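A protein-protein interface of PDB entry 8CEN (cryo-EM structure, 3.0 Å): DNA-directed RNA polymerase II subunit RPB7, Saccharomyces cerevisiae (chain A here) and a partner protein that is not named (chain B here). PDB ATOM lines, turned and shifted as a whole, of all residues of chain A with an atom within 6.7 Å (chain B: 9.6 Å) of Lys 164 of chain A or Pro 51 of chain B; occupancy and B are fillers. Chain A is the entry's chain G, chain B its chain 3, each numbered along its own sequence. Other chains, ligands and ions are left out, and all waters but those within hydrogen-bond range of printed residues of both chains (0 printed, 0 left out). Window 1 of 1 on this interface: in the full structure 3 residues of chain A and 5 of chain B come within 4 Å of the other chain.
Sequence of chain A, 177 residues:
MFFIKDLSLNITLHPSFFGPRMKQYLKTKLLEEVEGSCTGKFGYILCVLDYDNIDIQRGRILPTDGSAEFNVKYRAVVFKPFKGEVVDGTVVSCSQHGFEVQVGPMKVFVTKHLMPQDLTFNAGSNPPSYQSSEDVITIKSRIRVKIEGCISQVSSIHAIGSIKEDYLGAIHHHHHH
Of the 21 printed residues of chain B, 5 touch a printed residue of chain A.
Hydrophobic or aromatic side chains of chain B within 4 Å of the printed part of chain A: Leu 49 and Pro 51.
Among the printed residues, Asp or Glu carboxylates within 4 Å of a Lys or Arg side-chain nitrogen of the other chain: Asp 166 of chain A with Arg 64 of chain B (3.1 Å).
The backbone carbonyl oxygen of Ile 62 of chain B sits at hydrogen-bond distance from the guanidinium group of Arg 64 of chain B.
The side-chain carboxylate (OD2) of Asp 166 of chain A is in salt-bridge range of the guanidinium group (NE) of Arg 64 of chain B (3.1 Å).
OE2 of Glu 165 of chain A lies close to O of Leu 49 of chain B, at 2.9 Å.
The backbone NH (N) of Gly 50 of chain B sits close to the side-chain carboxylate (OE2) of Glu 165 of chain A, 3.3 Å away.
The side-chain carboxylate (OE2) of Glu 165 of chain A sits close to the backbone carbonyl oxygen (O) of Ser 48 of chain B (3.0 Å).
Among the printed residues, merely in contact across the chains: Lys 164 of chain A with Leu 49 of chain B (3.7 Å), Lys 164 of chain A with Pro 51 of chain B (3.4 Å) and Asp 166 of chain A with Pro 51 of chain B (3.3 Å).
Of chain B, only Leu 49 (3.7 Å) and Pro 51 (3.4 Å) come within 4 Å of Lys 164 of chain A.
Of the printed residues of chain A, Ser 48 of chain B touches Glu 165 (3.0 Å).
Of the printed residues of chain A, Leu 49 of chain B touches Lys 164 and Glu 165.
Pro 51 of chain B touches just these residues of chain A: Lys 164 and Asp 166.
The nearest residue of chain B that does not touch Lys 164 of chain A is Gly 50 of chain B (4.3 Å).
The nearest printed residue of chain A that does not touch Arg 64 of chain B is Glu 165 of chain A (7.0 Å).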
ATOM      1  N   HIS A 113      -5.444  -0.323 -20.140  1.00  0.00           N
ATOM      2  CA  HIS A 113      -5.184  -1.007 -21.399  1.00  0.00           C
ATOM      3  C   HIS A 113      -3.711  -1.009 -21.789  1.00  0.00           C
ATOM      4  O   HIS A 113      -3.350  -1.679 -22.763  1.00  0.00           O
ATOM      5  CB  HIS A 113      -6.000  -0.369 -22.528  1.00  0.00           C
ATOM      6  CG  HIS A 113      -7.466  -0.272 -22.239  1.00  0.00           C
ATOM      7  ND1 HIS A 113      -8.060   0.884 -21.781  1.00  0.00           N
ATOM      8  CD2 HIS A 113      -8.462  -1.181 -22.365  1.00  0.00           C
ATOM      9  CE1 HIS A 113      -9.356   0.680 -21.627  1.00  0.00           C
ATOM     10  NE2 HIS A 113      -9.627  -0.563 -21.977  1.00  0.00           N
ATOM     11  N   LEU A 114      -2.856  -0.284 -21.071  1.00  0.00           N
ATOM     12  CA  LEU A 114      -1.467  -0.082 -21.473  1.00  0.00           C
ATOM     13  C   LEU A 114      -0.483  -0.603 -20.429  1.00  0.00           C
ATOM     14  O   LEU A 114       0.511   0.051 -20.104  1.00  0.00           O
ATOM     15  CB  LEU A 114      -1.205   1.390 -21.781  1.00  0.00           C
ATOM     16  CG  LEU A 114      -2.159   2.004 -22.809  1.00  0.00           C
ATOM     17  CD1 LEU A 114      -1.796   3.442 -23.094  1.00  0.00           C
ATOM     18  CD2 LEU A 114      -2.141   1.194 -24.098  1.00  0.00           C
ATOM     19  N   MET A 115      -0.750  -1.785 -19.894  1.00  0.00           N
ATOM     20  CA  MET A 115       0.230  -2.594 -19.187  1.00  0.00           C
ATOM     21  C   MET A 115       0.251  -3.978 -19.812  1.00  0.00           C
ATOM     22  O   MET A 115      -0.697  -4.367 -20.502  1.00  0.00           O
ATOM     23  CB  MET A 115      -0.062  -2.717 -17.681  1.00  0.00           C
ATOM     24  CG  MET A 115       0.294  -1.500 -16.846  1.00  0.00           C
ATOM     25  SD  MET A 115      -0.813  -0.109 -17.032  1.00  0.00           S
ATOM     26  CE  MET A 115      -2.208  -0.729 -16.104  1.00  0.00           C
ATOM     27  N   PRO A 116       1.340  -4.734 -19.627  1.00  0.00           N
ATOM     28  CA  PRO A 116       1.325  -6.148 -20.020  1.00  0.00           C
ATOM     29  C   PRO A 116       0.252  -6.927 -19.272  1.00  0.00           C
ATOM     30  O   PRO A 116      -0.079  -6.628 -18.122  1.00  0.00           O
ATOM     31  CB  PRO A 116       2.732  -6.633 -19.655  1.00  0.00           C
ATOM     32  CG  PRO A 116       3.572  -5.412 -19.742  1.00  0.00           C
ATOM     33  CD  PRO A 116       2.700  -4.282 -19.277  1.00  0.00           C
ATOM     34  N   GLN A 117      -0.297  -7.936 -19.955  1.00  0.00           N
ATOM     35  CA  GLN A 117      -1.499  -8.621 -19.490  1.00  0.00           C
ATOM     36  C   GLN A 117      -1.274  -9.442 -18.226  1.00  0.00           C
ATOM     37  O   GLN A 117      -2.248  -9.773 -17.542  1.00  0.00           O
ATOM     38  CB  GLN A 117      -2.056  -9.523 -20.601  1.00  0.00           C
ATOM     39  CG  GLN A 117      -2.856  -8.824 -21.727  1.00  0.00           C
ATOM     40  CD  GLN A 117      -2.108  -7.723 -22.481  1.00  0.00           C
ATOM     41  OE1 GLN A 117      -0.879  -7.633 -22.443  1.00  0.00           O
ATOM     42  NE2 GLN A 117      -2.863  -6.875 -23.172  1.00  0.00           N
ATOM     43  N   SER A 162       2.490   4.633 -21.214  1.00  0.00           N
ATOM     44  CA  SER A 162       2.391   3.205 -21.477  1.00  0.00           C
ATOM     45  C   SER A 162       3.725   2.554 -21.148  1.00  0.00           C
ATOM     46  O   SER A 162       4.782   3.156 -21.351  1.00  0.00           O
ATOM     47  CB  SER A 162       2.007   2.922 -22.933  1.00  0.00           C
ATOM     48  OG  SER A 162       3.078   3.226 -23.810  1.00  0.00           O
ATOM     49  N   ILE A 163       3.666   1.325 -20.637  1.00  0.00           N
ATOM     50  CA  ILE A 163       4.871   0.575 -20.300  1.00  0.00           C
ATOM     51  C   ILE A 163       4.830  -0.781 -20.993  1.00  0.00           C
ATOM     52  O   ILE A 163       5.519  -1.722 -20.580  1.00  0.00           O
ATOM     53  CB  ILE A 163       5.024   0.409 -18.776  1.00  0.00           C
ATOM     54  CG1 ILE A 163       3.764  -0.220 -18.178  1.00  0.00           C
ATOM     55  CG2 ILE A 163       5.329   1.748 -18.110  1.00  0.00           C
ATOM     56  CD1 ILE A 163       3.933  -0.675 -16.747  1.00  0.00           C
ATOM     57  N   LYS A 164       4.026  -0.891 -22.054  1.00  0.00           N
ATOM     58  CA  LYS A 164       3.909  -2.154 -22.775  1.00  0.00           C
ATOM     59  C   LYS A 164       5.136  -2.451 -23.624  1.00  0.00           C
ATOM     60  O   LYS A 164       5.338  -3.606 -24.016  1.00  0.00           O
ATOM     61  CB  LYS A 164       2.653  -2.154 -23.645  1.00  0.00           C
ATOM     62  CG  LYS A 164       1.375  -2.371 -22.854  1.00  0.00           C
ATOM     63  CD  LYS A 164       0.218  -2.786 -23.745  1.00  0.00           C
ATOM     64  CE  LYS A 164       0.474  -4.142 -24.380  1.00  0.00           C
ATOM     65  NZ  LYS A 164      -0.758  -4.688 -25.008  1.00  0.00           N
ATOM     66  N   GLU A 165       5.942  -1.441 -23.934  1.00  0.00           N
ATOM     67  CA  GLU A 165       7.212  -1.675 -24.603  1.00  0.00           C
ATOM     68  C   GLU A 165       8.188  -2.373 -23.662  1.00  0.00           C
ATOM     69  O   GLU A 165       8.159  -2.181 -22.444  1.00  0.00           O
ATOM     70  CB  GLU A 165       7.816  -0.356 -25.091  1.00  0.00           C
ATOM     71  CG  GLU A 165       7.037   0.357 -26.192  1.00  0.00           C
ATOM     72  CD  GLU A 165       7.029  -0.406 -27.503  1.00  0.00           C
ATOM     73  OE1 GLU A 165       8.020  -1.107 -27.795  1.00  0.00           O
ATOM     74  OE2 GLU A 165       6.038  -0.287 -28.251  1.00  0.00           O
ATOM     75  N   ASP A 166       9.052  -3.202 -24.245  1.00  0.00           N
ATOM     76  CA  ASP A 166      10.083  -3.879 -23.474  1.00  0.00           C
ATOM     77  C   ASP A 166      11.107  -2.880 -22.947  1.00  0.00           C
ATOM     78  O   ASP A 166      11.301  -1.800 -23.512  1.00  0.00           O
ATOM     79  CB  ASP A 166      10.777  -4.945 -24.322  1.00  0.00           C
ATOM     80  CG  ASP A 166      10.037  -6.269 -24.311  1.00  0.00           C
ATOM     81  OD1 ASP A 166       9.628  -6.709 -23.217  1.00  0.00           O
ATOM     82  OD2 ASP A 166       9.868  -6.870 -25.394  1.00  0.00           O
ATOM     83  N   LEU A 168      10.869  -1.169 -20.244  1.00  0.00           N
ATOM     84  CA  LEU A 168      10.188  -0.100 -19.526  1.00  0.00           C
ATOM     85  C   LEU A 168       9.662  -0.648 -18.201  1.00  0.00           C
ATOM     86  O   LEU A 168       9.952  -1.784 -17.813  1.00  0.00           O
ATOM     87  CB  LEU A 168       9.057   0.501 -20.365  1.00  0.00           C
ATOM     88  CG  LEU A 168       9.384   1.621 -21.354  1.00  0.00           C
ATOM     89  CD1 LEU A 168      10.101   1.106 -22.585  1.00  0.00           C
ATOM     90  CD2 LEU A 168       8.112   2.349 -21.744  1.00  0.00           C
ATOM     91  N   ASN B  31      10.309 -11.452 -40.158  1.00  0.00           N
ATOM     92  CA  ASN B  31      11.042 -11.396 -38.905  1.00  0.00           C
ATOM     93  C   ASN B  31      12.023 -12.560 -38.814  1.00  0.00           C
ATOM     94  O   ASN B  31      11.717 -13.664 -39.278  1.00  0.00           O
ATOM     95  CB  ASN B  31      10.090 -11.439 -37.700  1.00  0.00           C
ATOM     96  CG  ASN B  31      10.601 -10.623 -36.528  1.00  0.00           C
ATOM     97  OD1 ASN B  31      11.030  -9.481 -36.693  1.00  0.00           O
ATOM     98  ND2 ASN B  31      10.583 -11.216 -35.342  1.00  0.00           N
ATOM     99  N   GLU B  33      12.931 -14.292 -36.191  1.00  0.00           N
ATOM    100  CA  GLU B  33      12.497 -15.357 -35.294  1.00  0.00           C
ATOM    101  C   GLU B  33      11.401 -16.210 -35.926  1.00  0.00           C
ATOM    102  O   GLU B  33      11.377 -17.432 -35.740  1.00  0.00           O
ATOM    103  CB  GLU B  33      12.044 -14.764 -33.960  1.00  0.00           C
ATOM    104  CG  GLU B  33      11.644 -15.794 -32.917  1.00  0.00           C
ATOM    105  CD  GLU B  33      11.261 -15.160 -31.597  1.00  0.00           C
ATOM    106  OE1 GLU B  33      11.291 -13.915 -31.509  1.00  0.00           O
ATOM    107  OE2 GLU B  33      10.931 -15.905 -30.650  1.00  0.00           O
ATOM    108  N   VAL B  43       2.436  -4.428 -39.658  1.00  0.00           N
ATOM    109  CA  VAL B  43       3.476  -4.271 -38.641  1.00  0.00           C
ATOM    110  C   VAL B  43       3.237  -3.006 -37.823  1.00  0.00           C
ATOM    111  O   VAL B  43       3.261  -3.031 -36.587  1.00  0.00           O
ATOM    112  CB  VAL B  43       4.869  -4.270 -39.296  1.00  0.00           C
ATOM    113  CG1 VAL B  43       5.932  -3.817 -38.307  1.00  0.00           C
ATOM    114  CG2 VAL B  43       5.208  -5.656 -39.825  1.00  0.00           C
ATOM    115  N   ILE B  46       0.067  -3.439 -35.513  1.00  0.00           N
ATOM    116  CA  ILE B  46       0.164  -4.321 -34.353  1.00  0.00           C
ATOM    117  C   ILE B  46       1.308  -3.918 -33.429  1.00  0.00           C
ATOM    118  O   ILE B  46       1.084  -3.579 -32.262  1.00  0.00           O
ATOM    119  CB  ILE B  46       0.320  -5.793 -34.778  1.00  0.00           C
ATOM    120  CG1 ILE B  46      -0.764  -6.182 -35.780  1.00  0.00           C
ATOM    121  CG2 ILE B  46       0.262  -6.707 -33.561  1.00  0.00           C
ATOM    122  CD1 ILE B  46      -0.510  -7.498 -36.481  1.00  0.00           C
ATOM    123  N   PHE B  47       2.537  -3.955 -33.935  1.00  0.00           N
ATOM    124  CA  PHE B  47       3.712  -3.980 -33.074  1.00  0.00           C
ATOM    125  C   PHE B  47       4.214  -2.594 -32.687  1.00  0.00           C
ATOM    126  O   PHE B  47       5.189  -2.497 -31.935  1.00  0.00           O
ATOM    127  CB  PHE B  47       4.856  -4.769 -33.735  1.00  0.00           C
ATOM    128  CG  PHE B  47       4.452  -6.123 -34.270  1.00  0.00           C
ATOM    129  CD1 PHE B  47       3.870  -6.260 -35.526  1.00  0.00           C
ATOM    130  CD2 PHE B  47       4.629  -7.258 -33.499  1.00  0.00           C
ATOM    131  CE1 PHE B  47       3.495  -7.502 -36.003  1.00  0.00           C
ATOM    132  CE2 PHE B  47       4.251  -8.499 -33.970  1.00  0.00           C
ATOM    133  CZ  PHE B  47       3.687  -8.622 -35.223  1.00  0.00           C
ATOM    134  N   SER B  48       3.585  -1.525 -33.181  1.00  0.00           N
ATOM    135  CA  SER B  48       4.013  -0.182 -32.799  1.00  0.00           C
ATOM    136  C   SER B  48       3.684   0.113 -31.340  1.00  0.00           C
ATOM    137  O   SER B  48       4.478   0.748 -30.635  1.00  0.00           O
ATOM    138  CB  SER B  48       3.366   0.859 -33.713  1.00  0.00           C
ATOM    139  OG  SER B  48       3.887   0.781 -35.029  1.00  0.00           O
ATOM    140  N   LEU B  49       2.515  -0.336 -30.874  1.00  0.00           N
ATOM    141  CA  LEU B  49       2.122  -0.098 -29.488  1.00  0.00           C
ATOM    142  C   LEU B  49       2.972  -0.915 -28.522  1.00  0.00           C
ATOM    143  O   LEU B  49       3.296  -0.449 -27.423  1.00  0.00           O
ATOM    144  CB  LEU B  49       0.634  -0.407 -29.312  1.00  0.00           C
ATOM    145  CG  LEU B  49      -0.029  -0.056 -27.978  1.00  0.00           C
ATOM    146  CD1 LEU B  49      -1.397   0.554 -28.220  1.00  0.00           C
ATOM    147  CD2 LEU B  49      -0.160  -1.287 -27.094  1.00  0.00           C
ATOM    148  N   GLY B  50       3.333  -2.136 -28.907  1.00  0.00           N
ATOM    149  CA  GLY B  50       4.177  -2.978 -28.094  1.00  0.00           C
ATOM    150  C   GLY B  50       4.416  -4.326 -28.739  1.00  0.00           C
ATOM    151  O   GLY B  50       3.832  -4.652 -29.777  1.00  0.00           O
ATOM    152  N   PRO B  51       5.299  -5.131 -28.147  1.00  0.00           N
ATOM    153  CA  PRO B  51       5.529  -6.483 -28.670  1.00  0.00           C
ATOM    154  C   PRO B  51       4.305  -7.366 -28.489  1.00  0.00           C
ATOM    155  O   PRO B  51       3.542  -7.225 -27.529  1.00  0.00           O
ATOM    156  CB  PRO B  51       6.710  -6.993 -27.836  1.00  0.00           C
ATOM    157  CG  PRO B  51       7.345  -5.759 -27.264  1.00  0.00           C
ATOM    158  CD  PRO B  51       6.222  -4.798 -27.050  1.00  0.00           C
ATOM    159  N   ALA B  52       4.119  -8.287 -29.432  1.00  0.00           N
ATOM    160  CA  ALA B  52       2.946  -9.148 -29.437  1.00  0.00           C
ATOM    161  C   ALA B  52       3.314 -10.491 -30.052  1.00  0.00           C
ATOM    162  O   ALA B  52       4.466 -10.736 -30.422  1.00  0.00           O
ATOM    163  CB  ALA B  52       1.785  -8.492 -30.190  1.00  0.00           C
ATOM    164  N   GLN B  53       2.318 -11.361 -30.160  1.00  0.00           N
ATOM    165  CA  GLN B  53       2.484 -12.698 -30.706  1.00  0.00           C
ATOM    166  C   GLN B  53       2.180 -12.702 -32.204  1.00  0.00           C
ATOM    167  O   GLN B  53       1.588 -11.765 -32.745  1.00  0.00           O
ATOM    168  CB  GLN B  53       1.602 -13.685 -29.927  1.00  0.00           C
ATOM    169  CG  GLN B  53       0.085 -13.456 -29.992  1.00  0.00           C
ATOM    170  CD  GLN B  53      -0.578 -14.069 -31.208  1.00  0.00           C
ATOM    171  OE1 GLN B  53      -0.121 -15.087 -31.724  1.00  0.00           O
ATOM    172  NE2 GLN B  53      -1.659 -13.453 -31.673  1.00  0.00           N
ATOM    173  N   CYS B  54       2.615 -13.767 -32.873  1.00  0.00           N
ATOM    174  CA  CYS B  54       2.548 -13.840 -34.335  1.00  0.00           C
ATOM    175  C   CYS B  54       1.104 -13.943 -34.806  1.00  0.00           C
ATOM    176  O   CYS B  54       0.418 -14.915 -34.465  1.00  0.00           O
ATOM    177  CB  CYS B  54       3.353 -15.036 -34.835  1.00  0.00           C
ATOM    178  SG  CYS B  54       3.535 -15.129 -36.633  1.00  0.00           S
ATOM    179  N   PRO B  55       0.612 -12.992 -35.608  1.00  0.00           N
ATOM    180  CA  PRO B  55      -0.819 -12.975 -35.961  1.00  0.00           C
ATOM    181  C   PRO B  55      -1.267 -14.125 -36.853  1.00  0.00           C
ATOM    182  O   PRO B  55      -2.477 -14.368 -36.945  1.00  0.00           O
ATOM    183  CB  PRO B  55      -0.986 -11.627 -36.676  1.00  0.00           C
ATOM    184  CG  PRO B  55       0.385 -11.282 -37.162  1.00  0.00           C
ATOM    185  CD  PRO B  55       1.329 -11.818 -36.134  1.00  0.00           C
ATOM    186  N   LYS B  61       4.682 -17.066 -31.314  1.00  0.00           N
ATOM    187  CA  LYS B  61       5.975 -16.578 -30.856  1.00  0.00           C
ATOM    188  C   LYS B  61       5.927 -15.077 -30.599  1.00  0.00           C
ATOM    189  O   LYS B  61       5.337 -14.318 -31.372  1.00  0.00           O
ATOM    190  CB  LYS B  61       7.063 -16.892 -31.883  1.00  0.00           C
ATOM    191  CG  LYS B  61       7.358 -18.373 -32.049  1.00  0.00           C
ATOM    192  CD  LYS B  61       8.484 -18.597 -33.045  1.00  0.00           C
ATOM    193  CE  LYS B  61       8.732 -20.078 -33.277  1.00  0.00           C
ATOM    194  NZ  LYS B  61       9.278 -20.748 -32.065  1.00  0.00           N
ATOM    195  N   ILE B  62       6.555 -14.655 -29.500  1.00  0.00           N
ATOM    196  CA  ILE B  62       6.677 -13.233 -29.201  1.00  0.00           C
ATOM    197  C   ILE B  62       7.747 -12.621 -30.098  1.00  0.00           C
ATOM    198  O   ILE B  62       8.778 -13.245 -30.386  1.00  0.00           O
ATOM    199  CB  ILE B  62       6.976 -13.030 -27.702  1.00  0.00           C
ATOM    200  CG1 ILE B  62       6.976 -11.545 -27.325  1.00  0.00           C
ATOM    201  CG2 ILE B  62       8.270 -13.728 -27.276  1.00  0.00           C
ATOM    202  CD1 ILE B  62       5.603 -10.917 -27.320  1.00  0.00           C
ATOM    203  N   LEU B  63       7.488 -11.409 -30.587  1.00  0.00           N
ATOM    204  CA  LEU B  63       8.397 -10.759 -31.522  1.00  0.00           C
ATOM    205  C   LEU B  63       8.223  -9.249 -31.433  1.00  0.00           C
ATOM    206  O   LEU B  63       7.166  -8.755 -31.035  1.00  0.00           O
ATOM    207  CB  LEU B  63       8.184 -11.261 -32.961  1.00  0.00           C
ATOM    208  CG  LEU B  63       6.956 -10.886 -33.797  1.00  0.00           C
ATOM    209  CD1 LEU B  63       7.211 -11.198 -35.257  1.00  0.00           C
ATOM    210  CD2 LEU B  63       5.729 -11.659 -33.344  1.00  0.00           C
ATOM    211  N   ARG B  64       9.276  -8.527 -31.812  1.00  0.00           N
ATOM    212  CA  ARG B  64       9.369  -7.086 -31.617  1.00  0.00           C
ATOM    213  C   ARG B  64       9.228  -6.344 -32.940  1.00  0.00           C
ATOM    214  O   ARG B  64       9.376  -6.916 -34.022  1.00  0.00           O
ATOM    215  CB  ARG B  64      10.701  -6.708 -30.957  1.00  0.00           C
ATOM    216  CG  ARG B  64      11.220  -7.719 -29.945  1.00  0.00           C
ATOM    217  CD  ARG B  64      10.342  -7.780 -28.705  1.00  0.00           C
ATOM    218  NE  ARG B  64      10.925  -8.621 -27.665  1.00  0.00           N
ATOM    219  CZ  ARG B  64      10.816  -9.941 -27.619  1.00  0.00           C
ATOM    220  NH1 ARG B  64      10.144 -10.612 -28.540  1.00  0.00           N
ATOM    221  NH2 ARG B  64      11.395 -10.606 -26.622  1.00  0.00           N
ATOM    222  N   LYS B  65       8.942  -5.042 -32.832  1.00  0.00           N
ATOM    223  CA  LYS B  65       8.750  -4.216 -34.021  1.00  0.00           C
ATOM    224  C   LYS B  65      10.080  -3.900 -34.696  1.00  0.00           C
ATOM    225  O   LYS B  65      10.176  -3.920 -35.928  1.00  0.00           O
ATOM    226  CB  LYS B  65       8.001  -2.932 -33.640  1.00  0.00           C
ATOM    227  CG  LYS B  65       7.553  -2.020 -34.798  1.00  0.00           C
ATOM    228  CD  LYS B  65       8.569  -0.940 -35.174  1.00  0.00           C
ATOM    229  CE  LYS B  65       8.035  -0.032 -36.269  1.00  0.00           C
ATOM    230  NZ  LYS B  65       9.031   1.001 -36.667  1.00  0.00           N
ATOM    231  N   ASN B  66      11.114  -3.599 -33.907  1.00  0.00           N
ATOM    232  CA  ASN B  66      12.379  -3.140 -34.467  1.00  0.00           C
ATOM    233  C   ASN B  66      13.186  -4.253 -35.121  1.00  0.00           C
ATOM    234  O   ASN B  66      14.174  -3.957 -35.801  1.00  0.00           O
ATOM    235  CB  ASN B  66      13.217  -2.464 -33.379  1.00  0.00           C
ATOM    236  CG  ASN B  66      13.727  -3.443 -32.342  1.00  0.00           C
ATOM    237  OD1 ASN B  66      13.032  -4.387 -31.966  1.00  0.00           O
ATOM    238  ND2 ASN B  66      14.949  -3.221 -31.870  1.00  0.00           N
ATOM    239  N   LYS B  67      12.800  -5.514 -34.937  1.00  0.00           N
ATOM    240  CA  LYS B  67      13.506  -6.627 -35.553  1.00  0.00           C
ATOM    241  C   LYS B  67      13.008  -6.953 -36.955  1.00  0.00           C
ATOM    242  O   LYS B  67      13.628  -7.779 -37.633  1.00  0.00           O
ATOM    243  CB  LYS B  67      13.397  -7.876 -34.671  1.00  0.00           C
ATOM    244  CG  LYS B  67      14.021  -7.713 -33.294  1.00  0.00           C
ATOM    245  CD  LYS B  67      15.495  -7.344 -33.396  1.00  0.00           C
ATOM    246  CE  LYS B  67      16.120  -7.180 -32.019  1.00  0.00           C
ATOM    247  NZ  LYS B  67      17.566  -6.835 -32.103  1.00  0.00           N
ATOM    248  N   PHE B  68      11.916  -6.335 -37.403  1.00  0.00           N
ATOM    249  CA  PHE B  68      11.415  -6.579 -38.749  1.00  0.00           C
ATOM    250  C   PHE B  68      12.372  -6.038 -39.805  1.00  0.00           C
ATOM    251  O   PHE B  68      13.060  -5.033 -39.604  1.00  0.00           O
ATOM    252  CB  PHE B  68      10.035  -5.950 -38.944  1.00  0.00           C
ATOM    253  CG  PHE B  68       8.916  -6.717 -38.299  1.00  0.00           C
ATOM    254  CD1 PHE B  68       8.369  -7.823 -38.930  1.00  0.00           C
ATOM    255  CD2 PHE B  68       8.393  -6.321 -37.078  1.00  0.00           C
ATOM    256  CE1 PHE B  68       7.335  -8.531 -38.351  1.00  0.00           C
ATOM    257  CE2 PHE B  68       7.356  -7.025 -36.494  1.00  0.00           C
ATOM    258  CZ  PHE B  68       6.827  -8.131 -37.132  1.00  0.00           C
